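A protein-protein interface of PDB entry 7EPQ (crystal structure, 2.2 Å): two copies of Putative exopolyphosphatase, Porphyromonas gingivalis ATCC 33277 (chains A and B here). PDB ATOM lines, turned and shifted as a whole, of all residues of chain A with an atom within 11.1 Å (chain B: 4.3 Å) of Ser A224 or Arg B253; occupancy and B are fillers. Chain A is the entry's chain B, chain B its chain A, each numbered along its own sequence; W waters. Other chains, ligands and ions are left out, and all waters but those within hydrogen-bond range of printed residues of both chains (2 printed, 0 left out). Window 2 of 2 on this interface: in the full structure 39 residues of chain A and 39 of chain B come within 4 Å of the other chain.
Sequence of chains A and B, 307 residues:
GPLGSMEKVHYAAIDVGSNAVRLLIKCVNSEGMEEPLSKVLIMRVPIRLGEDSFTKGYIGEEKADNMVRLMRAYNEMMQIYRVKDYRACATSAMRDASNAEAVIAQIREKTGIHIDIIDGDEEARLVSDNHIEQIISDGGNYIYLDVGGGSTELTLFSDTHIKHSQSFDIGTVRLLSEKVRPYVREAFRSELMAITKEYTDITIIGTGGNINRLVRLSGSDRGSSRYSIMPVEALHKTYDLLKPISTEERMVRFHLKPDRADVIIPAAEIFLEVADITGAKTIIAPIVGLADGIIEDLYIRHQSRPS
O of Ser A224 lies within hydrogen-bond range of NH1 of Arg B253 (3.0 Å).
A ring nitrogen (ND1) of His B255 sits close to the guanidinium group (NE) of Arg A222, 3.3 Å away.
A ring nitrogen (NE2) of His B255 sits at hydrogen-bond distance from the guanidinium group (NH1) of Arg A226 (3.2 Å).
The side-chain amide nitrogen (ND2) of Asn A29 sits at hydrogen-bond distance from the backbone carbonyl oxygen (O) of Glu A35 (3.3 Å).
ND2 of Asn A29 sits at hydrogen-bond distance from OG of Ser A38, at 2.5 Å.
OE2 of Glu A35 sits at hydrogen-bond distance from NE2 of His A131 (2.9 Å).
O of Arg A226 sits at hydrogen-bond distance from NH1 of Arg A222, at 3.5 Å.
N of Arg A222 sits at hydrogen-bond distance from OG of Ser A228, at 3.1 Å.
Among the printed residues, merely in contact across the chains: Gly A223 with Leu B217, Ser A224 with Leu B217, Ser A38 with Met B251, Ser A225 with His B255, Glu A35 with Val B252 and Ser A224 with Phe B254.
Of chain B, only Leu B217 (3.4 Å), Arg B253 (3.0 Å) and Phe B254 (3.9 Å) come within 4 Å of Ser A224.
Of chain A, only Glu A35 comes within 4 Å of Val B252.
Of chain A, only Ser A224 comes within 4 Å of Phe B254.
Of the printed residues of chain B, Ser A225 touches His B255.
Of the printed residues of chain B, Arg A222 touches His B255.
Of the printed residues of chain B, Ser A38 touches Met B251 (3.4 Å).
Printed residues of chain A within 4 Å of His B255: Arg A222 (3.3 Å), Ser A225 (3.6 Å) and Arg A226 (3.0 Å).
The nearest printed residue of chain A that does not touch Arg B253 is Ser A225 (4.01 Å).
The nearest printed residue of chain B that does not touch Ser A225 is Arg B253 (4.01 Å).
Of the 8 printed residues of chain B, 6 touch a printed residue of chain A.
Printed residues of chain B that touch a printed residue of chain A: Leu B217, Met B251, Val B252, Arg B253, Phe B254 and His B255.
Hydrophobic or aromatic side chains of chain B that line the printed part of chain A: Leu B217, Met B251, Val B252, Phe B254 and His B255.
Along chain A the printed residues that touch a printed residue of chain B span positions 35 to 226.
Among the printed residues, no Asp or Glu carboxylate lies within 4 Å of a Lys or Arg side-chain nitrogen of the other chain.
No position is printed for both chains.
Of the 9 pairs that touch across the chains among the printed residues, none has its exchanged pair printed and touching as well.
Water W2 lies within hydrogen-bond range of O of Val B252 (2.4 Å) and OE1 of Glu A35 (3.0 Å).
Water W1 lies within hydrogen-bond range of the backbone NH (N) of Ser A224 (2.8 Å), the backbone carbonyl oxygen (O) of Arg A222 (3.1 Å) and the backbone carbonyl oxygen (O) of Leu B217 (3.4 Å).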
ATOM      1  N   ASN A  29       1.809  15.527 -23.521  1.00  0.00           N
ATOM      2  CA  ASN A  29       1.243  16.699 -22.868  1.00  0.00           C
ATOM      3  C   ASN A  29       2.330  17.437 -22.089  1.00  0.00           C
ATOM      4  O   ASN A  29       3.527  17.202 -22.270  1.00  0.00           O
ATOM      5  CB  ASN A  29       0.103  16.282 -21.943  1.00  0.00           C
ATOM      6  CG  ASN A  29      -0.926  15.423 -22.636  1.00  0.00           C
ATOM      7  OD1 ASN A  29      -1.201  15.601 -23.830  1.00  0.00           O
ATOM      8  ND2 ASN A  29      -1.515  14.484 -21.889  1.00  0.00           N
ATOM      9  N   GLU A  35      -1.842  13.232 -16.629  1.00  0.00           N
ATOM     10  CA  GLU A  35      -1.343  12.360 -17.689  1.00  0.00           C
ATOM     11  C   GLU A  35      -0.234  13.029 -18.481  1.00  0.00           C
ATOM     12  O   GLU A  35      -0.344  14.194 -18.864  1.00  0.00           O
ATOM     13  CB  GLU A  35      -2.463  11.938 -18.661  1.00  0.00           C
ATOM     14  CG  GLU A  35      -3.373  10.765 -18.231  1.00  0.00           C
ATOM     15  CD  GLU A  35      -4.409  10.406 -19.324  1.00  0.00           C
ATOM     16  OE1 GLU A  35      -4.598  11.222 -20.262  1.00  0.00           O
ATOM     17  OE2 GLU A  35      -5.019   9.307 -19.263  1.00  0.00           O
ATOM     18  N   PRO A  36       0.845  12.285 -18.734  1.00  0.00           N
ATOM     19  CA  PRO A  36       1.866  12.772 -19.672  1.00  0.00           C
ATOM     20  C   PRO A  36       1.517  12.552 -21.143  1.00  0.00           C
ATOM     21  O   PRO A  36       2.121  13.202 -22.008  1.00  0.00           O
ATOM     22  CB  PRO A  36       3.106  11.961 -19.275  1.00  0.00           C
ATOM     23  CG  PRO A  36       2.533  10.657 -18.775  1.00  0.00           C
ATOM     24  CD  PRO A  36       1.232  11.018 -18.087  1.00  0.00           C
ATOM     25  N   LEU A  37       0.563  11.674 -21.458  1.00  0.00           N
ATOM     26  CA  LEU A  37       0.268  11.272 -22.830  1.00  0.00           C
ATOM     27  C   LEU A  37      -1.237  11.288 -23.047  1.00  0.00           C
ATOM     28  O   LEU A  37      -1.985  10.757 -22.221  1.00  0.00           O
ATOM     29  CB  LEU A  37       0.816   9.866 -23.121  1.00  0.00           C
ATOM     30  CG  LEU A  37       2.342   9.716 -23.134  1.00  0.00           C
ATOM     31  CD1 LEU A  37       2.742   8.339 -22.619  1.00  0.00           C
ATOM     32  CD2 LEU A  37       2.901   9.968 -24.535  1.00  0.00           C
ATOM     33  N   SER A  38      -1.680  11.865 -24.161  1.00  0.00           N
ATOM     34  CA  SER A  38      -3.101  11.896 -24.490  1.00  0.00           C
ATOM     35  C   SER A  38      -3.357  11.258 -25.849  1.00  0.00           C
ATOM     36  O   SER A  38      -2.572  11.430 -26.793  1.00  0.00           O
ATOM     37  CB  SER A  38      -3.640  13.327 -24.466  1.00  0.00           C
ATOM     38  OG  SER A  38      -3.571  13.867 -23.149  1.00  0.00           O
ATOM     39  N   LYS A  39      -4.456  10.513 -25.931  1.00  0.00           N
ATOM     40  CA  LYS A  39      -4.861   9.878 -27.179  1.00  0.00           C
ATOM     41  C   LYS A  39      -5.347  10.924 -28.174  1.00  0.00           C
ATOM     42  O   LYS A  39      -6.179  11.772 -27.838  1.00  0.00           O
ATOM     43  CB  LYS A  39      -5.967   8.856 -26.892  1.00  0.00           C
ATOM     44  CG  LYS A  39      -6.572   8.210 -28.111  1.00  0.00           C
ATOM     45  CD  LYS A  39      -7.311   6.903 -27.768  1.00  0.00           C
ATOM     46  CE  LYS A  39      -8.511   7.150 -26.872  1.00  0.00           C
ATOM     47  NZ  LYS A  39      -9.184   5.867 -26.493  1.00  0.00           N
ATOM     48  N   HIS A 131      -1.329   3.901 -15.827  1.00  0.00           N
ATOM     49  CA  HIS A 131      -2.744   3.817 -15.479  1.00  0.00           C
ATOM     50  C   HIS A 131      -2.995   2.723 -14.448  1.00  0.00           C
ATOM     51  O   HIS A 131      -3.797   2.905 -13.527  1.00  0.00           O
ATOM     52  CB  HIS A 131      -3.580   3.571 -16.738  1.00  0.00           C
ATOM     53  CG  HIS A 131      -3.653   4.756 -17.642  1.00  0.00           C
ATOM     54  ND1 HIS A 131      -2.909   4.851 -18.796  1.00  0.00           N
ATOM     55  CD2 HIS A 131      -4.355   5.910 -17.550  1.00  0.00           C
ATOM     56  CE1 HIS A 131      -3.155   6.008 -19.383  1.00  0.00           C
ATOM     57  NE2 HIS A 131      -4.026   6.671 -18.644  1.00  0.00           N
ATOM     58  N   GLY A 219     -24.899  -0.130 -19.424  1.00  0.00           N
ATOM     59  CA  GLY A 219     -25.166   1.103 -18.718  1.00  0.00           C
ATOM     60  C   GLY A 219     -24.077   1.548 -17.763  1.00  0.00           C
ATOM     61  O   GLY A 219     -24.373   2.249 -16.794  1.00  0.00           O
ATOM     62  N   SER A 220     -22.813   1.190 -18.019  1.00  0.00           N
ATOM     63  CA  SER A 220     -21.725   1.580 -17.127  1.00  0.00           C
ATOM     64  C   SER A 220     -20.670   2.437 -17.830  1.00  0.00           C
ATOM     65  O   SER A 220     -19.518   2.498 -17.376  1.00  0.00           O
ATOM     66  CB  SER A 220     -21.080   0.342 -16.492  1.00  0.00           C
ATOM     67  OG  SER A 220     -22.067  -0.516 -15.912  1.00  0.00           O
ATOM     68  N   ASP A 221     -21.037   3.098 -18.928  1.00  0.00           N
ATOM     69  CA  ASP A 221     -20.155   4.072 -19.562  1.00  0.00           C
ATOM     70  C   ASP A 221     -19.656   5.075 -18.529  1.00  0.00           C
ATOM     71  O   ASP A 221     -20.394   5.466 -17.621  1.00  0.00           O
ATOM     72  CB  ASP A 221     -20.904   4.792 -20.682  1.00  0.00           C
ATOM     73  CG  ASP A 221     -19.978   5.482 -21.657  1.00  0.00           C
ATOM     74  OD1 ASP A 221     -18.999   4.849 -22.107  1.00  0.00           O
ATOM     75  OD2 ASP A 221     -20.234   6.658 -21.986  1.00  0.00           O
ATOM     76  N   ARG A 222     -18.381   5.466 -18.638  1.00  0.00           N
ATOM     77  CA  ARG A 222     -17.842   6.406 -17.656  1.00  0.00           C
ATOM     78  C   ARG A 222     -18.424   7.795 -17.861  1.00  0.00           C
ATOM     79  O   ARG A 222     -18.915   8.422 -16.911  1.00  0.00           O
ATOM     80  CB  ARG A 222     -16.309   6.449 -17.706  1.00  0.00           C
ATOM     81  CG  ARG A 222     -15.674   6.976 -18.995  1.00  0.00           C
ATOM     82  CD  ARG A 222     -14.159   7.034 -18.861  1.00  0.00           C
ATOM     83  NE  ARG A 222     -13.494   7.064 -20.164  1.00  0.00           N
ATOM     84  CZ  ARG A 222     -12.197   6.822 -20.349  1.00  0.00           C
ATOM     85  NH1 ARG A 222     -11.418   6.529 -19.316  1.00  0.00           N
ATOM     86  NH2 ARG A 222     -11.676   6.860 -21.572  1.00  0.00           N
ATOM     87  N   GLY A 223     -18.413   8.277 -19.107  1.00  0.00           N
ATOM     88  CA  GLY A 223     -18.805   9.640 -19.395  1.00  0.00           C
ATOM     89  C   GLY A 223     -17.941  10.630 -18.644  1.00  0.00           C
ATOM     90  O   GLY A 223     -16.747  10.781 -18.940  1.00  0.00           O
ATOM     91  N   SER A 224     -18.525  11.285 -17.644  1.00  0.00           N
ATOM     92  CA  SER A 224     -17.804  12.301 -16.886  1.00  0.00           C
ATOM     93  C   SER A 224     -17.044  11.736 -15.685  1.00  0.00           C
ATOM     94  O   SER A 224     -16.351  12.495 -15.004  1.00  0.00           O
ATOM     95  CB  SER A 224     -18.772  13.411 -16.443  1.00  0.00           C
ATOM     96  OG  SER A 224     -19.718  12.935 -15.499  1.00  0.00           O
ATOM     97  N   SER A 225     -17.134  10.431 -15.418  1.00  0.00           N
ATOM     98  CA  SER A 225     -16.352   9.824 -14.346  1.00  0.00           C
ATOM     99  C   SER A 225     -14.922   9.555 -14.815  1.00  0.00           C
ATOM    100  O   SER A 225     -14.597   9.659 -16.001  1.00  0.00           O
ATOM    101  CB  SER A 225     -17.001   8.524 -13.868  1.00  0.00           C
ATOM    102  OG  SER A 225     -18.095   8.787 -13.006  1.00  0.00           O
ATOM    103  N   ARG A 226     -14.053   9.198 -13.864  1.00  0.00           N
ATOM    104  CA  ARG A 226     -12.685   8.845 -14.231  1.00  0.00           C
ATOM    105  C   ARG A 226     -12.635   7.488 -14.923  1.00  0.00           C
ATOM    106  O   ARG A 226     -11.985   7.336 -15.963  1.00  0.00           O
ATOM    107  CB  ARG A 226     -11.781   8.851 -13.001  1.00  0.00           C
ATOM    108  CG  ARG A 226     -10.327   8.463 -13.315  1.00  0.00           C
ATOM    109  CD  ARG A 226      -9.778   9.251 -14.506  1.00  0.00           C
ATOM    110  NE  ARG A 226      -8.318   9.361 -14.486  1.00  0.00           N
ATOM    111  CZ  ARG A 226      -7.504   8.770 -15.361  1.00  0.00           C
ATOM    112  NH1 ARG A 226      -7.998   8.033 -16.348  1.00  0.00           N
ATOM    113  NH2 ARG A 226      -6.192   8.931 -15.259  1.00  0.00           N
ATOM    114  N   TYR A 227     -13.321   6.492 -14.367  1.00  0.00           N
ATOM    115  CA  TYR A 227     -13.302   5.140 -14.910  1.00  0.00           C
ATOM    116  C   TYR A 227     -14.715   4.628 -15.122  1.00  0.00           C
ATOM    117  O   TYR A 227     -15.640   4.979 -14.381  1.00  0.00           O
ATOM    118  CB  TYR A 227     -12.592   4.160 -13.981  1.00  0.00           C
ATOM    119  CG  TYR A 227     -11.196   4.542 -13.588  1.00  0.00           C
ATOM    120  CD1 TYR A 227     -10.142   4.429 -14.489  1.00  0.00           C
ATOM    121  CD2 TYR A 227     -10.921   4.989 -12.300  1.00  0.00           C
ATOM    122  CE1 TYR A 227      -8.850   4.768 -14.118  1.00  0.00           C
ATOM    123  CE2 TYR A 227      -9.636   5.327 -11.921  1.00  0.00           C
ATOM    124  CZ  TYR A 227      -8.607   5.214 -12.831  1.00  0.00           C
ATOM    125  OH  TYR A 227      -7.335   5.558 -12.445  1.00  0.00           O
ATOM    126  N   SER A 228     -14.869   3.772 -16.127  1.00  0.00           N
ATOM    127  CA  SER A 228     -16.070   2.961 -16.256  1.00  0.00           C
ATOM    128  C   SER A 228     -15.975   1.797 -15.279  1.00  0.00           C
ATOM    129  O   SER A 228     -14.953   1.110 -15.230  1.00  0.00           O
ATOM    130  CB  SER A 228     -16.220   2.423 -17.675  1.00  0.00           C
ATOM    131  OG  SER A 228     -16.080   3.451 -18.636  1.00  0.00           O
ATOM    132  N   ILE A 229     -17.036   1.570 -14.506  1.00  0.00           N
ATOM    133  CA  ILE A 229     -17.045   0.540 -13.473  1.00  0.00           C
ATOM    134  C   ILE A 229     -18.330  -0.240 -13.645  1.00  0.00           C
ATOM    135  O   ILE A 229     -19.421   0.310 -13.455  1.00  0.00           O
ATOM    136  CB  ILE A 229     -16.942   1.132 -12.063  1.00  0.00           C
ATOM    137  CG1 ILE A 229     -15.629   1.897 -11.922  1.00  0.00           C
ATOM    138  CG2 ILE A 229     -17.022   0.039 -11.020  1.00  0.00           C
ATOM    139  CD1 ILE A 229     -15.563   2.807 -10.737  1.00  0.00           C
ATOM    140  N   PRO A 286     -10.496   0.624 -17.794  1.00  0.00           N
ATOM    141  CA  PRO A 286      -9.813   1.911 -17.963  1.00  0.00           C
ATOM    142  C   PRO A 286      -9.592   2.330 -19.412  1.00  0.00           C
ATOM    143  O   PRO A 286      -9.022   3.400 -19.638  1.00  0.00           O
ATOM    144  CB  PRO A 286      -8.468   1.675 -17.263  1.00  0.00           C
ATOM    145  CG  PRO A 286      -8.217   0.215 -17.439  1.00  0.00           C
ATOM    146  CD  PRO A 286      -9.569  -0.458 -17.423  1.00  0.00           C
ATOM    147  N   ILE A 287     -10.007   1.522 -20.391  1.00  0.00           N
ATOM    148  CA  ILE A 287      -9.965   1.886 -21.810  1.00  0.00           C
ATOM    149  C   ILE A 287      -8.517   2.137 -22.209  1.00  0.00           C
ATOM    150  O   ILE A 287      -8.200   3.133 -22.871  1.00  0.00           O
ATOM    151  CB  ILE A 287     -10.837   3.116 -22.141  1.00  0.00           C
ATOM    152  CG1 ILE A 287     -12.141   3.136 -21.323  1.00  0.00           C
ATOM    153  CG2 ILE A 287     -11.172   3.154 -23.632  1.00  0.00           C
ATOM    154  CD1 ILE A 287     -12.989   1.880 -21.420  1.00  0.00           C
ATOM    155  N   LEU B 217     -20.829  12.384 -22.041  1.00  0.00           N
ATOM    156  CA  LEU B 217     -20.388  13.094 -20.842  1.00  0.00           C
ATOM    157  C   LEU B 217     -21.548  13.410 -19.912  1.00  0.00           C
ATOM    158  O   LEU B 217     -21.358  13.492 -18.694  1.00  0.00           O
ATOM    159  CB  LEU B 217     -19.661  14.384 -21.224  1.00  0.00           C
ATOM    160  CG  LEU B 217     -18.282  14.137 -21.838  1.00  0.00           C
ATOM    161  CD1 LEU B 217     -17.693  15.401 -22.430  1.00  0.00           C
ATOM    162  CD2 LEU B 217     -17.351  13.533 -20.793  1.00  0.00           C
ATOM    163  N   GLU B 249      -6.934  20.810 -19.577  1.00  0.00           N
ATOM    164  CA  GLU B 249      -7.548  20.179 -18.410  1.00  0.00           C
ATOM    165  C   GLU B 249      -8.819  19.432 -18.798  1.00  0.00           C
ATOM    166  O   GLU B 249      -9.117  18.375 -18.231  1.00  0.00           O
ATOM    167  CB  GLU B 249      -7.857  21.220 -17.328  1.00  0.00           C
ATOM    168  CG  GLU B 249      -6.805  22.308 -17.170  1.00  0.00           C
ATOM    169  CD  GLU B 249      -7.235  23.435 -16.219  1.00  0.00           C
ATOM    170  OE1 GLU B 249      -6.355  23.989 -15.520  1.00  0.00           O
ATOM    171  OE2 GLU B 249      -8.438  23.772 -16.175  1.00  0.00           O
ATOM    172  N   ARG B 250      -9.597  19.977 -19.741  1.00  0.00           N
ATOM    173  CA  ARG B 250     -10.757  19.245 -20.244  1.00  0.00           C
ATOM    174  C   ARG B 250     -10.326  17.941 -20.892  1.00  0.00           C
ATOM    175  O   ARG B 250     -10.943  16.889 -20.673  1.00  0.00           O
ATOM    176  CB  ARG B 250     -11.550  20.091 -21.239  1.00  0.00           C
ATOM    177  CG  ARG B 250     -12.493  21.040 -20.585  1.00  0.00           C
ATOM    178  CD  ARG B 250     -13.563  21.522 -21.526  1.00  0.00           C
ATOM    179  NE  ARG B 250     -13.002  22.346 -22.580  1.00  0.00           N
ATOM    180  CZ  ARG B 250     -12.887  23.664 -22.526  1.00  0.00           C
ATOM    181  NH1 ARG B 250     -13.298  24.325 -21.459  1.00  0.00           N
ATOM    182  NH2 ARG B 250     -12.358  24.315 -23.554  1.00  0.00           N
ATOM    183  N   MET B 251      -9.263  17.995 -21.700  1.00  0.00           N
ATOM    184  CA  MET B 251      -8.689  16.797 -22.299  1.00  0.00           C
ATOM    185  C   MET B 251      -8.483  15.706 -21.271  1.00  0.00           C
ATOM    186  O   MET B 251      -9.083  14.629 -21.347  1.00  0.00           O
ATOM    187  CB  MET B 251      -7.338  17.107 -22.941  1.00  0.00           C
ATOM    188  CG  MET B 251      -7.360  17.852 -24.227  1.00  0.00           C
ATOM    189  SD  MET B 251      -5.643  18.183 -24.643  1.00  0.00           S
ATOM    190  CE  MET B 251      -5.040  16.502 -24.788  1.00  0.00           C
ATOM    191  N   VAL B 252      -7.622  15.994 -20.297  1.00  0.00           N
ATOM    192  CA  VAL B 252      -7.141  14.966 -19.384  1.00  0.00           C
ATOM    193  C   VAL B 252      -8.249  14.534 -18.434  1.00  0.00           C
ATOM    194  O   VAL B 252      -8.510  13.335 -18.270  1.00  0.00           O
ATOM    195  CB  VAL B 252      -5.901  15.473 -18.625  1.00  0.00           C
ATOM    196  CG1 VAL B 252      -5.360  14.387 -17.722  1.00  0.00           C
ATOM    197  CG2 VAL B 252      -4.834  15.927 -19.607  1.00  0.00           C
ATOM    198  N   ARG B 253      -8.924  15.501 -17.805  1.00  0.00           N
ATOM    199  CA  ARG B 253      -9.949  15.168 -16.814  1.00  0.00           C
ATOM    200  C   ARG B 253     -11.120  14.392 -17.424  1.00  0.00           C
ATOM    201  O   ARG B 253     -11.698  13.522 -16.760  1.00  0.00           O
ATOM    202  CB  ARG B 253     -10.444  16.445 -16.129  1.00  0.00           C
ATOM    203  CG  ARG B 253     -11.698  16.282 -15.291  1.00  0.00           C
ATOM    204  CD  ARG B 253     -11.502  15.273 -14.166  1.00  0.00           C
ATOM    205  NE  ARG B 253     -12.707  15.113 -13.344  1.00  0.00           N
ATOM    206  CZ  ARG B 253     -13.648  14.189 -13.546  1.00  0.00           C
ATOM    207  NH1 ARG B 253     -13.540  13.315 -14.549  1.00  0.00           N
ATOM    208  NH2 ARG B 253     -14.700  14.137 -12.738  1.00  0.00           N
ATOM    209  N   PHE B 254     -11.474  14.660 -18.682  1.00  0.00           N
ATOM    210  CA  PHE B 254     -12.669  14.063 -19.264  1.00  0.00           C
ATOM    211  C   PHE B 254     -12.396  13.173 -20.468  1.00  0.00           C
ATOM    212  O   PHE B 254     -13.350  12.786 -21.156  1.00  0.00           O
ATOM    213  CB  PHE B 254     -13.665  15.156 -19.646  1.00  0.00           C
ATOM    214  CG  PHE B 254     -14.171  15.930 -18.476  1.00  0.00           C
ATOM    215  CD1 PHE B 254     -15.001  15.329 -17.544  1.00  0.00           C
ATOM    216  CD2 PHE B 254     -13.812  17.250 -18.296  1.00  0.00           C
ATOM    217  CE1 PHE B 254     -15.477  16.039 -16.454  1.00  0.00           C
ATOM    218  CE2 PHE B 254     -14.281  17.967 -17.208  1.00  0.00           C
ATOM    219  CZ  PHE B 254     -15.119  17.361 -16.286  1.00  0.00           C
ATOM    220  N   HIS B 255     -11.131  12.837 -20.738  1.00  0.00           N
ATOM    221  CA  HIS B 255     -10.771  11.876 -21.783  1.00  0.00           C
ATOM    222  C   HIS B 255     -11.274  12.337 -23.150  1.00  0.00           C
ATOM    223  O   HIS B 255     -11.989  11.623 -23.857  1.00  0.00           O
ATOM    224  CB  HIS B 255     -11.302  10.485 -21.436  1.00  0.00           C
ATOM    225  CG  HIS B 255     -11.054  10.092 -20.013  1.00  0.00           C
ATOM    226  ND1 HIS B 255     -12.075   9.853 -19.116  1.00  0.00           N
ATOM    227  CD2 HIS B 255      -9.897   9.898 -19.329  1.00  0.00           C
ATOM    228  CE1 HIS B 255     -11.559   9.537 -17.940  1.00  0.00           C
ATOM    229  NE2 HIS B 255     -10.241   9.556 -18.042  1.00  0.00           N
HETATM  230  O   HOH W   1     -21.111  10.621 -16.915  1.00  0.00           O
HETATM  231  O   HOH W   2      -7.542  11.554 -19.580  1.00  0.00           O
